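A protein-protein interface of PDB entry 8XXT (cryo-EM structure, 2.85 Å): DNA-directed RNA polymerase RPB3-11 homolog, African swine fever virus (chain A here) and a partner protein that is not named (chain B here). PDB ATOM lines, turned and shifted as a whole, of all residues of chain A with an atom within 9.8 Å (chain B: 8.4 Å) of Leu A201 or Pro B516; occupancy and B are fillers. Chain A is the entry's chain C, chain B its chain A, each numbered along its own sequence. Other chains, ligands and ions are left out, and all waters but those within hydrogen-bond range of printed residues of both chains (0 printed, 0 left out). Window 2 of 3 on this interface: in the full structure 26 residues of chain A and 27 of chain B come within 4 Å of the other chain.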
ATOM      1  N   GLN A 190      -4.590  -7.673  -0.384  1.00  0.00           N
ATOM      2  CA  GLN A 190      -5.980  -7.934  -0.049  1.00  0.00           C
ATOM      3  C   GLN A 190      -6.805  -8.123  -1.311  1.00  0.00           C
ATOM      4  O   GLN A 190      -6.618  -7.410  -2.301  1.00  0.00           O
ATOM      5  CB  GLN A 190      -6.571  -6.795   0.777  1.00  0.00           C
ATOM      6  CG  GLN A 190      -5.863  -6.532   2.079  1.00  0.00           C
ATOM      7  CD  GLN A 190      -6.773  -5.893   3.098  1.00  0.00           C
ATOM      8  OE1 GLN A 190      -7.860  -6.397   3.373  1.00  0.00           O
ATOM      9  NE2 GLN A 190      -6.338  -4.774   3.663  1.00  0.00           N
ATOM     10  N   TYR A 191      -7.717  -9.089  -1.267  1.00  0.00           N
ATOM     11  CA  TYR A 191      -8.682  -9.260  -2.334  1.00  0.00           C
ATOM     12  C   TYR A 191      -9.717  -8.142  -2.287  1.00  0.00           C
ATOM     13  O   TYR A 191      -9.926  -7.517  -1.245  1.00  0.00           O
ATOM     14  CB  TYR A 191      -9.394 -10.603  -2.209  1.00  0.00           C
ATOM     15  CG  TYR A 191      -8.535 -11.807  -2.483  1.00  0.00           C
ATOM     16  CD1 TYR A 191      -7.727 -11.864  -3.605  1.00  0.00           C
ATOM     17  CD2 TYR A 191      -8.550 -12.897  -1.630  1.00  0.00           C
ATOM     18  CE1 TYR A 191      -6.948 -12.968  -3.862  1.00  0.00           C
ATOM     19  CE2 TYR A 191      -7.776 -14.004  -1.878  1.00  0.00           C
ATOM     20  CZ  TYR A 191      -6.976 -14.034  -2.996  1.00  0.00           C
ATOM     21  OH  TYR A 191      -6.199 -15.139  -3.248  1.00  0.00           O
ATOM     22  N   PRO A 192     -10.379  -7.865  -3.408  1.00  0.00           N
ATOM     23  CA  PRO A 192     -11.573  -7.017  -3.348  1.00  0.00           C
ATOM     24  C   PRO A 192     -12.738  -7.790  -2.753  1.00  0.00           C
ATOM     25  O   PRO A 192     -13.329  -8.648  -3.416  1.00  0.00           O
ATOM     26  CB  PRO A 192     -11.815  -6.642  -4.814  1.00  0.00           C
ATOM     27  CG  PRO A 192     -11.179  -7.738  -5.591  1.00  0.00           C
ATOM     28  CD  PRO A 192     -10.005  -8.208  -4.791  1.00  0.00           C
ATOM     29  N   THR A 193     -13.075  -7.496  -1.498  1.00  0.00           N
ATOM     30  CA  THR A 193     -14.053  -8.292  -0.769  1.00  0.00           C
ATOM     31  C   THR A 193     -15.489  -7.998  -1.179  1.00  0.00           C
ATOM     32  O   THR A 193     -16.378  -8.794  -0.865  1.00  0.00           O
ATOM     33  CB  THR A 193     -13.894  -8.072   0.734  1.00  0.00           C
ATOM     34  OG1 THR A 193     -13.965  -6.671   1.024  1.00  0.00           O
ATOM     35  CG2 THR A 193     -12.555  -8.605   1.200  1.00  0.00           C
ATOM     36  N   ASP A 194     -15.738  -6.886  -1.871  1.00  0.00           N
ATOM     37  CA  ASP A 194     -17.070  -6.623  -2.398  1.00  0.00           C
ATOM     38  C   ASP A 194     -17.450  -7.572  -3.525  1.00  0.00           C
ATOM     39  O   ASP A 194     -18.618  -7.596  -3.923  1.00  0.00           O
ATOM     40  CB  ASP A 194     -17.173  -5.173  -2.873  1.00  0.00           C
ATOM     41  CG  ASP A 194     -15.935  -4.711  -3.614  1.00  0.00           C
ATOM     42  OD1 ASP A 194     -14.817  -5.072  -3.189  1.00  0.00           O
ATOM     43  OD2 ASP A 194     -16.078  -3.982  -4.618  1.00  0.00           O
ATOM     44  N   LYS A 195     -16.501  -8.346  -4.046  1.00  0.00           N
ATOM     45  CA  LYS A 195     -16.792  -9.332  -5.071  1.00  0.00           C
ATOM     46  C   LYS A 195     -17.447 -10.566  -4.455  1.00  0.00           C
ATOM     47  O   LYS A 195     -17.331 -10.831  -3.258  1.00  0.00           O
ATOM     48  CB  LYS A 195     -15.516  -9.724  -5.815  1.00  0.00           C
ATOM     49  CG  LYS A 195     -14.762  -8.545  -6.402  1.00  0.00           C
ATOM     50  CD  LYS A 195     -15.680  -7.666  -7.230  1.00  0.00           C
ATOM     51  CE  LYS A 195     -14.916  -6.533  -7.893  1.00  0.00           C
ATOM     52  NZ  LYS A 195     -14.140  -6.995  -9.074  1.00  0.00           N
ATOM     53  N   LYS A 196     -18.147 -11.323  -5.301  1.00  0.00           N
ATOM     54  CA  LYS A 196     -18.894 -12.478  -4.815  1.00  0.00           C
ATOM     55  C   LYS A 196     -17.974 -13.646  -4.484  1.00  0.00           C
ATOM     56  O   LYS A 196     -18.196 -14.357  -3.500  1.00  0.00           O
ATOM     57  CB  LYS A 196     -19.934 -12.900  -5.852  1.00  0.00           C
ATOM     58  CG  LYS A 196     -20.785 -14.087  -5.436  1.00  0.00           C
ATOM     59  CD  LYS A 196     -21.772 -13.705  -4.349  1.00  0.00           C
ATOM     60  CE  LYS A 196     -22.735 -12.638  -4.836  1.00  0.00           C
ATOM     61  NZ  LYS A 196     -23.916 -12.506  -3.945  1.00  0.00           N
ATOM     62  N   GLU A 197     -16.942 -13.867  -5.299  1.00  0.00           N
ATOM     63  CA  GLU A 197     -16.100 -15.043  -5.121  1.00  0.00           C
ATOM     64  C   GLU A 197     -15.173 -14.924  -3.920  1.00  0.00           C
ATOM     65  O   GLU A 197     -14.688 -15.946  -3.426  1.00  0.00           O
ATOM     66  CB  GLU A 197     -15.284 -15.298  -6.389  1.00  0.00           C
ATOM     67  CG  GLU A 197     -14.255 -14.224  -6.691  1.00  0.00           C
ATOM     68  CD  GLU A 197     -14.795 -13.128  -7.588  1.00  0.00           C
ATOM     69  OE1 GLU A 197     -15.879 -12.588  -7.285  1.00  0.00           O
ATOM     70  OE2 GLU A 197     -14.133 -12.805  -8.597  1.00  0.00           O
ATOM     71  N   TYR A 198     -14.915 -13.710  -3.441  1.00  0.00           N
ATOM     72  CA  TYR A 198     -14.039 -13.489  -2.298  1.00  0.00           C
ATOM     73  C   TYR A 198     -14.784 -12.958  -1.083  1.00  0.00           C
ATOM     74  O   TYR A 198     -14.147 -12.492  -0.135  1.00  0.00           O
ATOM     75  CB  TYR A 198     -12.914 -12.526  -2.678  1.00  0.00           C
ATOM     76  CG  TYR A 198     -12.111 -12.968  -3.875  1.00  0.00           C
ATOM     77  CD1 TYR A 198     -11.543 -14.229  -3.922  1.00  0.00           C
ATOM     78  CD2 TYR A 198     -11.915 -12.121  -4.952  1.00  0.00           C
ATOM     79  CE1 TYR A 198     -10.807 -14.637  -5.009  1.00  0.00           C
ATOM     80  CE2 TYR A 198     -11.180 -12.520  -6.044  1.00  0.00           C
ATOM     81  CZ  TYR A 198     -10.627 -13.779  -6.067  1.00  0.00           C
ATOM     82  OH  TYR A 198      -9.891 -14.187  -7.154  1.00  0.00           O
ATOM     83  N   MET A 199     -16.114 -13.008  -1.089  1.00  0.00           N
ATOM     84  CA  MET A 199     -16.881 -12.441   0.012  1.00  0.00           C
ATOM     85  C   MET A 199     -16.847 -13.325   1.251  1.00  0.00           C
ATOM     86  O   MET A 199     -17.010 -12.819   2.366  1.00  0.00           O
ATOM     87  CB  MET A 199     -18.322 -12.189  -0.435  1.00  0.00           C
ATOM     88  CG  MET A 199     -19.310 -13.274  -0.063  1.00  0.00           C
ATOM     89  SD  MET A 199     -21.013 -12.730  -0.269  1.00  0.00           S
ATOM     90  CE  MET A 199     -21.812 -14.273  -0.702  1.00  0.00           C
ATOM     91  N   ALA A 200     -16.630 -14.629   1.086  1.00  0.00           N
ATOM     92  CA  ALA A 200     -16.574 -15.535   2.225  1.00  0.00           C
ATOM     93  C   ALA A 200     -15.195 -15.609   2.858  1.00  0.00           C
ATOM     94  O   ALA A 200     -15.047 -16.250   3.903  1.00  0.00           O
ATOM     95  CB  ALA A 200     -17.012 -16.936   1.807  1.00  0.00           C
ATOM     96  N   LEU A 201     -14.190 -14.984   2.261  1.00  0.00           N
ATOM     97  CA  LEU A 201     -12.827 -15.013   2.763  1.00  0.00           C
ATOM     98  C   LEU A 201     -12.516 -13.733   3.526  1.00  0.00           C
ATOM     99  O   LEU A 201     -13.240 -12.741   3.439  1.00  0.00           O
ATOM    100  CB  LEU A 201     -11.836 -15.193   1.613  1.00  0.00           C
ATOM    101  CG  LEU A 201     -12.183 -16.317   0.642  1.00  0.00           C
ATOM    102  CD1 LEU A 201     -11.186 -16.368  -0.491  1.00  0.00           C
ATOM    103  CD2 LEU A 201     -12.216 -17.633   1.381  1.00  0.00           C
ATOM    104  N   SER A 202     -11.418 -13.769   4.283  1.00  0.00           N
ATOM    105  CA  SER A 202     -11.028 -12.596   5.055  1.00  0.00           C
ATOM    106  C   SER A 202     -10.667 -11.427   4.154  1.00  0.00           C
ATOM    107  O   SER A 202     -10.959 -10.274   4.485  1.00  0.00           O
ATOM    108  CB  SER A 202      -9.857 -12.932   5.971  1.00  0.00           C
ATOM    109  OG  SER A 202      -8.721 -13.313   5.221  1.00  0.00           O
ATOM    110  N   GLY A 203     -10.038 -11.701   3.013  1.00  0.00           N
ATOM    111  CA  GLY A 203      -9.595 -10.684   2.089  1.00  0.00           C
ATOM    112  C   GLY A 203      -8.104 -10.705   1.834  1.00  0.00           C
ATOM    113  O   GLY A 203      -7.672 -10.391   0.722  1.00  0.00           O
ATOM    114  N   TYR A 204      -7.312 -11.074   2.836  1.00  0.00           N
ATOM    115  CA  TYR A 204      -5.872 -11.155   2.655  1.00  0.00           C
ATOM    116  C   TYR A 204      -5.528 -12.279   1.691  1.00  0.00           C
ATOM    117  O   TYR A 204      -6.144 -13.346   1.714  1.00  0.00           O
ATOM    118  CB  TYR A 204      -5.180 -11.385   3.994  1.00  0.00           C
ATOM    119  CG  TYR A 204      -5.104 -10.150   4.848  1.00  0.00           C
ATOM    120  CD1 TYR A 204      -4.516  -8.995   4.373  1.00  0.00           C
ATOM    121  CD2 TYR A 204      -5.631 -10.137   6.125  1.00  0.00           C
ATOM    122  CE1 TYR A 204      -4.449  -7.865   5.145  1.00  0.00           C
ATOM    123  CE2 TYR A 204      -5.568  -9.014   6.905  1.00  0.00           C
ATOM    124  CZ  TYR A 204      -4.976  -7.878   6.411  1.00  0.00           C
ATOM    125  OH  TYR A 204      -4.912  -6.750   7.188  1.00  0.00           O
ATOM    126  N   LYS A 205      -4.540 -12.034   0.834  1.00  0.00           N
ATOM    127  CA  LYS A 205      -4.177 -13.026  -0.169  1.00  0.00           C
ATOM    128  C   LYS A 205      -3.394 -14.188   0.425  1.00  0.00           C
ATOM    129  O   LYS A 205      -3.465 -15.305  -0.095  1.00  0.00           O
ATOM    130  CB  LYS A 205      -3.378 -12.364  -1.290  1.00  0.00           C
ATOM    131  CG  LYS A 205      -4.172 -11.344  -2.082  1.00  0.00           C
ATOM    132  CD  LYS A 205      -3.680 -11.251  -3.510  1.00  0.00           C
ATOM    133  CE  LYS A 205      -4.547 -10.316  -4.329  1.00  0.00           C
ATOM    134  NZ  LYS A 205      -3.978  -8.945  -4.384  1.00  0.00           N
ATOM    135  N   GLN A 206      -2.648 -13.953   1.498  1.00  0.00           N
ATOM    136  CA  GLN A 206      -1.884 -15.004   2.152  1.00  0.00           C
ATOM    137  C   GLN A 206      -2.705 -15.642   3.262  1.00  0.00           C
ATOM    138  O   GLN A 206      -3.347 -14.946   4.052  1.00  0.00           O
ATOM    139  CB  GLN A 206      -0.587 -14.446   2.733  1.00  0.00           C
ATOM    140  CG  GLN A 206       0.355 -13.844   1.714  1.00  0.00           C
ATOM    141  CD  GLN A 206       1.534 -13.156   2.363  1.00  0.00           C
ATOM    142  OE1 GLN A 206       1.899 -13.462   3.496  1.00  0.00           O
ATOM    143  NE2 GLN A 206       2.135 -12.215   1.648  1.00  0.00           N
ATOM    144  N   SER A 207      -2.676 -16.967   3.321  1.00  0.00           N
ATOM    145  CA  SER A 207      -3.346 -17.673   4.402  1.00  0.00           C
ATOM    146  C   SER A 207      -2.688 -17.336   5.730  1.00  0.00           C
ATOM    147  O   SER A 207      -1.468 -17.191   5.816  1.00  0.00           O
ATOM    148  CB  SER A 207      -3.304 -19.178   4.161  1.00  0.00           C
ATOM    149  OG  SER A 207      -3.793 -19.886   5.284  1.00  0.00           O
ATOM    150  N   LEU B 509     -11.569 -29.759   8.199  1.00  0.00           N
ATOM    151  CA  LEU B 509     -10.865 -28.579   7.710  1.00  0.00           C
ATOM    152  C   LEU B 509      -9.359 -28.732   7.864  1.00  0.00           C
ATOM    153  O   LEU B 509      -8.594 -28.297   6.997  1.00  0.00           O
ATOM    154  CB  LEU B 509     -11.351 -27.331   8.441  1.00  0.00           C
ATOM    155  CG  LEU B 509     -12.824 -26.957   8.292  1.00  0.00           C
ATOM    156  CD1 LEU B 509     -13.133 -25.737   9.132  1.00  0.00           C
ATOM    157  CD2 LEU B 509     -13.185 -26.715   6.842  1.00  0.00           C
ATOM    158  N   ARG B 512      -8.296 -31.528   5.099  1.00  0.00           N
ATOM    159  CA  ARG B 512      -8.636 -31.400   3.691  1.00  0.00           C
ATOM    160  C   ARG B 512      -7.425 -30.933   2.896  1.00  0.00           C
ATOM    161  O   ARG B 512      -6.483 -30.352   3.440  1.00  0.00           O
ATOM    162  CB  ARG B 512      -9.808 -30.440   3.495  1.00  0.00           C
ATOM    163  CG  ARG B 512      -9.535 -29.031   3.940  1.00  0.00           C
ATOM    164  CD  ARG B 512     -10.702 -28.128   3.619  1.00  0.00           C
ATOM    165  NE  ARG B 512     -10.564 -26.828   4.263  1.00  0.00           N
ATOM    166  CZ  ARG B 512     -11.206 -25.733   3.885  1.00  0.00           C
ATOM    167  NH1 ARG B 512     -12.042 -25.741   2.862  1.00  0.00           N
ATOM    168  NH2 ARG B 512     -11.004 -24.601   4.551  1.00  0.00           N
ATOM    169  N   THR B 513      -7.451 -31.206   1.591  1.00  0.00           N
ATOM    170  CA  THR B 513      -6.278 -30.958   0.758  1.00  0.00           C
ATOM    171  C   THR B 513      -6.129 -29.480   0.425  1.00  0.00           C
ATOM    172  O   THR B 513      -5.068 -28.889   0.649  1.00  0.00           O
ATOM    173  CB  THR B 513      -6.361 -31.781  -0.524  1.00  0.00           C
ATOM    174  OG1 THR B 513      -6.577 -33.156  -0.193  1.00  0.00           O
ATOM    175  CG2 THR B 513      -5.076 -31.652  -1.313  1.00  0.00           C
ATOM    176  N   ASN B 514      -7.175 -28.870  -0.122  1.00  0.00           N
ATOM    177  CA  ASN B 514      -7.106 -27.515  -0.645  1.00  0.00           C
ATOM    178  C   ASN B 514      -8.062 -26.616   0.118  1.00  0.00           C
ATOM    179  O   ASN B 514      -9.250 -26.926   0.238  1.00  0.00           O
ATOM    180  CB  ASN B 514      -7.449 -27.485  -2.135  1.00  0.00           C
ATOM    181  CG  ASN B 514      -6.332 -28.015  -3.004  1.00  0.00           C
ATOM    182  OD1 ASN B 514      -6.403 -29.132  -3.513  1.00  0.00           O
ATOM    183  ND2 ASN B 514      -5.292 -27.214  -3.180  1.00  0.00           N
ATOM    184  N   THR B 515      -7.545 -25.524   0.626  1.00  0.00           N
ATOM    185  CA  THR B 515      -8.336 -24.422   1.141  1.00  0.00           C
ATOM    186  C   THR B 515      -8.685 -23.470   0.007  1.00  0.00           C
ATOM    187  O   THR B 515      -8.067 -23.513  -1.059  1.00  0.00           O
ATOM    188  CB  THR B 515      -7.561 -23.686   2.229  1.00  0.00           C
ATOM    189  OG1 THR B 515      -6.351 -23.157   1.678  1.00  0.00           O
ATOM    190  CG2 THR B 515      -7.218 -24.625   3.355  1.00  0.00           C
ATOM    191  N   PRO B 516      -9.682 -22.603   0.189  1.00  0.00           N
ATOM    192  CA  PRO B 516      -9.967 -21.605  -0.854  1.00  0.00           C
ATOM    193  C   PRO B 516      -8.789 -20.701  -1.154  1.00  0.00           C
ATOM    194  O   PRO B 516      -8.705 -20.164  -2.265  1.00  0.00           O
ATOM    195  CB  PRO B 516     -11.151 -20.817  -0.275  1.00  0.00           C
ATOM    196  CG  PRO B 516     -11.169 -21.147   1.180  1.00  0.00           C
ATOM    197  CD  PRO B 516     -10.668 -22.542   1.277  1.00  0.00           C
ATOM    198  N   MET B 517      -7.878 -20.510  -0.200  1.00  0.00           N
ATOM    199  CA  MET B 517      -6.664 -19.751  -0.463  1.00  0.00           C
ATOM    200  C   MET B 517      -5.693 -20.525  -1.342  1.00  0.00           C
ATOM    201  O   MET B 517      -4.999 -19.927  -2.170  1.00  0.00           O
ATOM    202  CB  MET B 517      -5.985 -19.382   0.854  1.00  0.00           C
ATOM    203  CG  MET B 517      -6.815 -18.474   1.732  1.00  0.00           C
ATOM    204  SD  MET B 517      -6.552 -16.719   1.444  1.00  0.00           S
ATOM    205  CE  MET B 517      -7.403 -16.044   2.869  1.00  0.00           C
ATOM    206  N   GLY B 518      -5.635 -21.839  -1.180  1.00  0.00           N
ATOM    207  CA  GLY B 518      -4.692 -22.675  -1.905  1.00  0.00           C
ATOM    208  C   GLY B 518      -4.548 -24.019  -1.210  1.00  0.00           C
ATOM    209  O   GLY B 518      -5.489 -24.513  -0.592  1.00  0.00           O
ATOM    210  N   LYS B 519      -3.356 -24.592  -1.333  1.00  0.00           N
ATOM    211  CA  LYS B 519      -3.065 -25.845  -0.650  1.00  0.00           C
ATOM    212  C   LYS B 519      -3.124 -25.648   0.860  1.00  0.00           C
ATOM    213  O   LYS B 519      -2.718 -24.608   1.384  1.00  0.00           O
ATOM    214  CB  LYS B 519      -1.692 -26.365  -1.065  1.00  0.00           C
ATOM    215  CG  LYS B 519      -1.510 -27.853  -0.871  1.00  0.00           C
ATOM    216  CD  LYS B 519      -0.821 -28.475  -2.070  1.00  0.00           C
ATOM    217  CE  LYS B 519      -1.806 -28.749  -3.194  1.00  0.00           C
ATOM    218  NZ  LYS B 519      -2.567 -30.010  -2.972  1.00  0.00           N
ATOM    219  N   ASN B 520      -3.640 -26.654   1.561  1.00  0.00           N
ATOM    220  CA  ASN B 520      -3.851 -26.566   3.005  1.00  0.00           C
ATOM    221  C   ASN B 520      -2.538 -26.869   3.712  1.00  0.00           C
ATOM    222  O   ASN B 520      -2.270 -27.997   4.123  1.00  0.00           O
ATOM    223  CB  ASN B 520      -4.952 -27.521   3.446  1.00  0.00           C
ATOM    224  CG  ASN B 520      -5.471 -27.212   4.829  1.00  0.00           C
ATOM    225  OD1 ASN B 520      -5.089 -26.217   5.441  1.00  0.00           O
ATOM    226  ND2 ASN B 520      -6.352 -28.064   5.330  1.00  0.00           N
ATOM    227  N   TYR B 643      -6.624 -25.611  14.922  1.00  0.00           N
ATOM    228  CA  TYR B 643      -6.591 -25.286  13.501  1.00  0.00           C
ATOM    229  C   TYR B 643      -7.660 -24.262  13.148  1.00  0.00           C
ATOM    230  O   TYR B 643      -7.391 -23.291  12.435  1.00  0.00           O
ATOM    231  CB  TYR B 643      -6.770 -26.548  12.665  1.00  0.00           C
ATOM    232  CG  TYR B 643      -6.773 -26.281  11.181  1.00  0.00           C
ATOM    233  CD1 TYR B 643      -5.587 -26.189  10.474  1.00  0.00           C
ATOM    234  CD2 TYR B 643      -7.961 -26.121  10.486  1.00  0.00           C
ATOM    235  CE1 TYR B 643      -5.584 -25.948   9.121  1.00  0.00           C
ATOM    236  CE2 TYR B 643      -7.964 -25.879   9.133  1.00  0.00           C
ATOM    237  CZ  TYR B 643      -6.773 -25.792   8.457  1.00  0.00           C
ATOM    238  OH  TYR B 643      -6.772 -25.551   7.105  1.00  0.00           O
ATOM    239  N   ALA B 647      -7.951 -20.959  10.923  1.00  0.00           N
ATOM    240  CA  ALA B 647      -8.741 -21.066   9.705  1.00  0.00           C
ATOM    241  C   ALA B 647     -10.072 -20.347   9.842  1.00  0.00           C
ATOM    242  O   ALA B 647     -10.545 -19.717   8.890  1.00  0.00           O
ATOM    243  CB  ALA B 647      -8.962 -22.534   9.352  1.00  0.00           C
ATOM    244  N   THR B 650     -17.668 -20.248  10.155  1.00  0.00           N
ATOM    245  CA  THR B 650     -18.844 -19.429  10.402  1.00  0.00           C
ATOM    246  C   THR B 650     -19.998 -19.929   9.551  1.00  0.00           C
ATOM    247  O   THR B 650     -19.815 -20.704   8.611  1.00  0.00           O
ATOM    248  CB  THR B 650     -18.580 -17.954  10.099  1.00  0.00           C
ATOM    249  OG1 THR B 650     -19.608 -17.156  10.693  1.00  0.00           O
ATOM    250  CG2 THR B 650     -18.582 -17.719   8.606  1.00  0.00           C
ATOM    251  N   ASN B 724     -20.950 -22.664  -2.508  1.00  0.00           N
ATOM    252  CA  ASN B 724     -19.522 -22.866  -2.693  1.00  0.00           C
ATOM    253  C   ASN B 724     -19.061 -23.824  -1.613  1.00  0.00           C
ATOM    254  O   ASN B 724     -18.816 -23.395  -0.477  1.00  0.00           O
ATOM    255  CB  ASN B 724     -18.758 -21.544  -2.607  1.00  0.00           C
ATOM    256  CG  ASN B 724     -17.298 -21.695  -2.969  1.00  0.00           C
ATOM    257  OD1 ASN B 724     -16.849 -22.773  -3.353  1.00  0.00           O
ATOM    258  ND2 ASN B 724     -16.544 -20.611  -2.843  1.00  0.00           N
ATOM    259  N   PRO B 725     -18.934 -25.119  -1.901  1.00  0.00           N
ATOM    260  CA  PRO B 725     -18.686 -26.089  -0.826  1.00  0.00           C
ATOM    261  C   PRO B 725     -17.395 -25.862  -0.065  1.00  0.00           C
ATOM    262  O   PRO B 725     -17.295 -26.278   1.095  1.00  0.00           O
ATOM    263  CB  PRO B 725     -18.665 -27.422  -1.576  1.00  0.00           C
ATOM    264  CG  PRO B 725     -19.441 -27.175  -2.810  1.00  0.00           C
ATOM    265  CD  PRO B 725     -19.105 -25.780  -3.201  1.00  0.00           C
ATOM    266  N   GLU B 726     -16.397 -25.227  -0.678  1.00  0.00           N
ATOM    267  CA  GLU B 726     -15.148 -24.987   0.031  1.00  0.00           C
ATOM    268  C   GLU B 726     -15.322 -23.981   1.158  1.00  0.00           C
ATOM    269  O   GLU B 726     -14.606 -24.053   2.161  1.00  0.00           O
ATOM    270  CB  GLU B 726     -14.071 -24.510  -0.940  1.00  0.00           C
ATOM    271  CG  GLU B 726     -13.588 -25.580  -1.900  1.00  0.00           C
ATOM    272  CD  GLU B 726     -12.200 -25.294  -2.436  1.00  0.00           C
ATOM    273  OE1 GLU B 726     -11.843 -24.104  -2.551  1.00  0.00           O
ATOM    274  OE2 GLU B 726     -11.468 -26.259  -2.746  1.00  0.00           O
ATOM    275  N   THR B 727     -16.261 -23.044   1.021  1.00  0.00           N
ATOM    276  CA  THR B 727     -16.441 -21.988   2.004  1.00  0.00           C
ATOM    277  C   THR B 727     -17.812 -21.966   2.663  1.00  0.00           C
ATOM    278  O   THR B 727     -17.984 -21.242   3.648  1.00  0.00           O
ATOM    279  CB  THR B 727     -16.190 -20.612   1.369  1.00  0.00           C
ATOM    280  OG1 THR B 727     -17.301 -20.260   0.538  1.00  0.00           O
ATOM    281  CG2 THR B 727     -14.926 -20.628   0.533  1.00  0.00           C
ATOM    282  N   ASN B 728     -18.784 -22.725   2.162  1.00  0.00           N
ATOM    283  CA  ASN B 728     -20.136 -22.689   2.712  1.00  0.00           C
ATOM    284  C   ASN B 728     -20.153 -23.366   4.073  1.00  0.00           C
ATOM    285  O   ASN B 728     -19.923 -24.574   4.176  1.00  0.00           O
ATOM    286  CB  ASN B 728     -21.111 -23.366   1.757  1.00  0.00           C
ATOM    287  CG  ASN B 728     -22.416 -22.616   1.630  1.00  0.00           C
ATOM    288  OD1 ASN B 728     -23.311 -22.760   2.460  1.00  0.00           O
ATOM    289  ND2 ASN B 728     -22.533 -21.804   0.588  1.00  0.00           N
ATOM    290  N   GLN B 732     -20.814 -27.536   4.842  1.00  0.00           N
ATOM    291  CA  GLN B 732     -19.729 -28.310   5.428  1.00  0.00           C
ATOM    292  C   GLN B 732     -20.166 -28.994   6.715  1.00  0.00           C
ATOM    293  O   GLN B 732     -19.772 -30.134   6.981  1.00  0.00           O
ATOM    294  CB  GLN B 732     -18.524 -27.408   5.672  1.00  0.00           C
ATOM    295  CG  GLN B 732     -17.810 -27.016   4.401  1.00  0.00           C
ATOM    296  CD  GLN B 732     -16.675 -26.061   4.647  1.00  0.00           C
ATOM    297  OE1 GLN B 732     -16.550 -25.492   5.728  1.00  0.00           O
ATOM    298  NE2 GLN B 732     -15.837 -25.873   3.640  1.00  0.00           N
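The side-chain sulfur (SD) of Met B517 sits close to the backbone carbonyl oxygen (O) of Tyr A204, at 3.4 Å.
The backbone carbonyl oxygen (O) of Lys A205 sits close to the side-chain sulfur (SD) of Met B517 (3.7 Å).
The side-chain amide nitrogen of Asn B724 sits at hydrogen-bond distance from the side-chain hydroxyl of Thr B727 (3.5 Å).
Pro B516 touches just one residue of chain A: Leu A201.
Ala A200 touches just one residue of chain B: Thr B727 (3.6 Å).
Ser A202 touches just one residue of chain B: Met B517 (3.8 Å).
Met B517 touches just these residues of chain A: Ser A202 (3.8 Å), Tyr A204 (3.2 Å) and Lys A205 (3.7 Å).
No residue of chain A comes within 4 Å of Gly B518.
Of the printed residues of chain B, Tyr A204 touches Met B517 (3.2 Å).
Of the printed residues of chain A, Thr B727 touches Ala A200 (3.6 Å).
Printed residues of chain B within 4 Å of Lys A205: Met B517.
Gln B732 touches none of the printed residues of chain A.
Lys A195 touches none of the printed residues of chain B.
Of the 18 printed residues of chain A, 5 touch a printed residue of chain B.
Printed residues of chain B that touch a printed residue of chain A: Pro B516, Met B517 and Thr B727.
Among the printed residues, 5 pairs touch across the chains.
Among the printed residues, no Asp or Glu carboxylate lies within 4 Å of a Lys or Arg side-chain nitrogen of the other chain.
Among the printed residues, pairs that only touch across the chains: Ala A200 with Thr B727 (3.6 Å), Leu A201 with Pro B516 (3.7 Å) and Ser A202 with Met B517 (3.8 Å).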
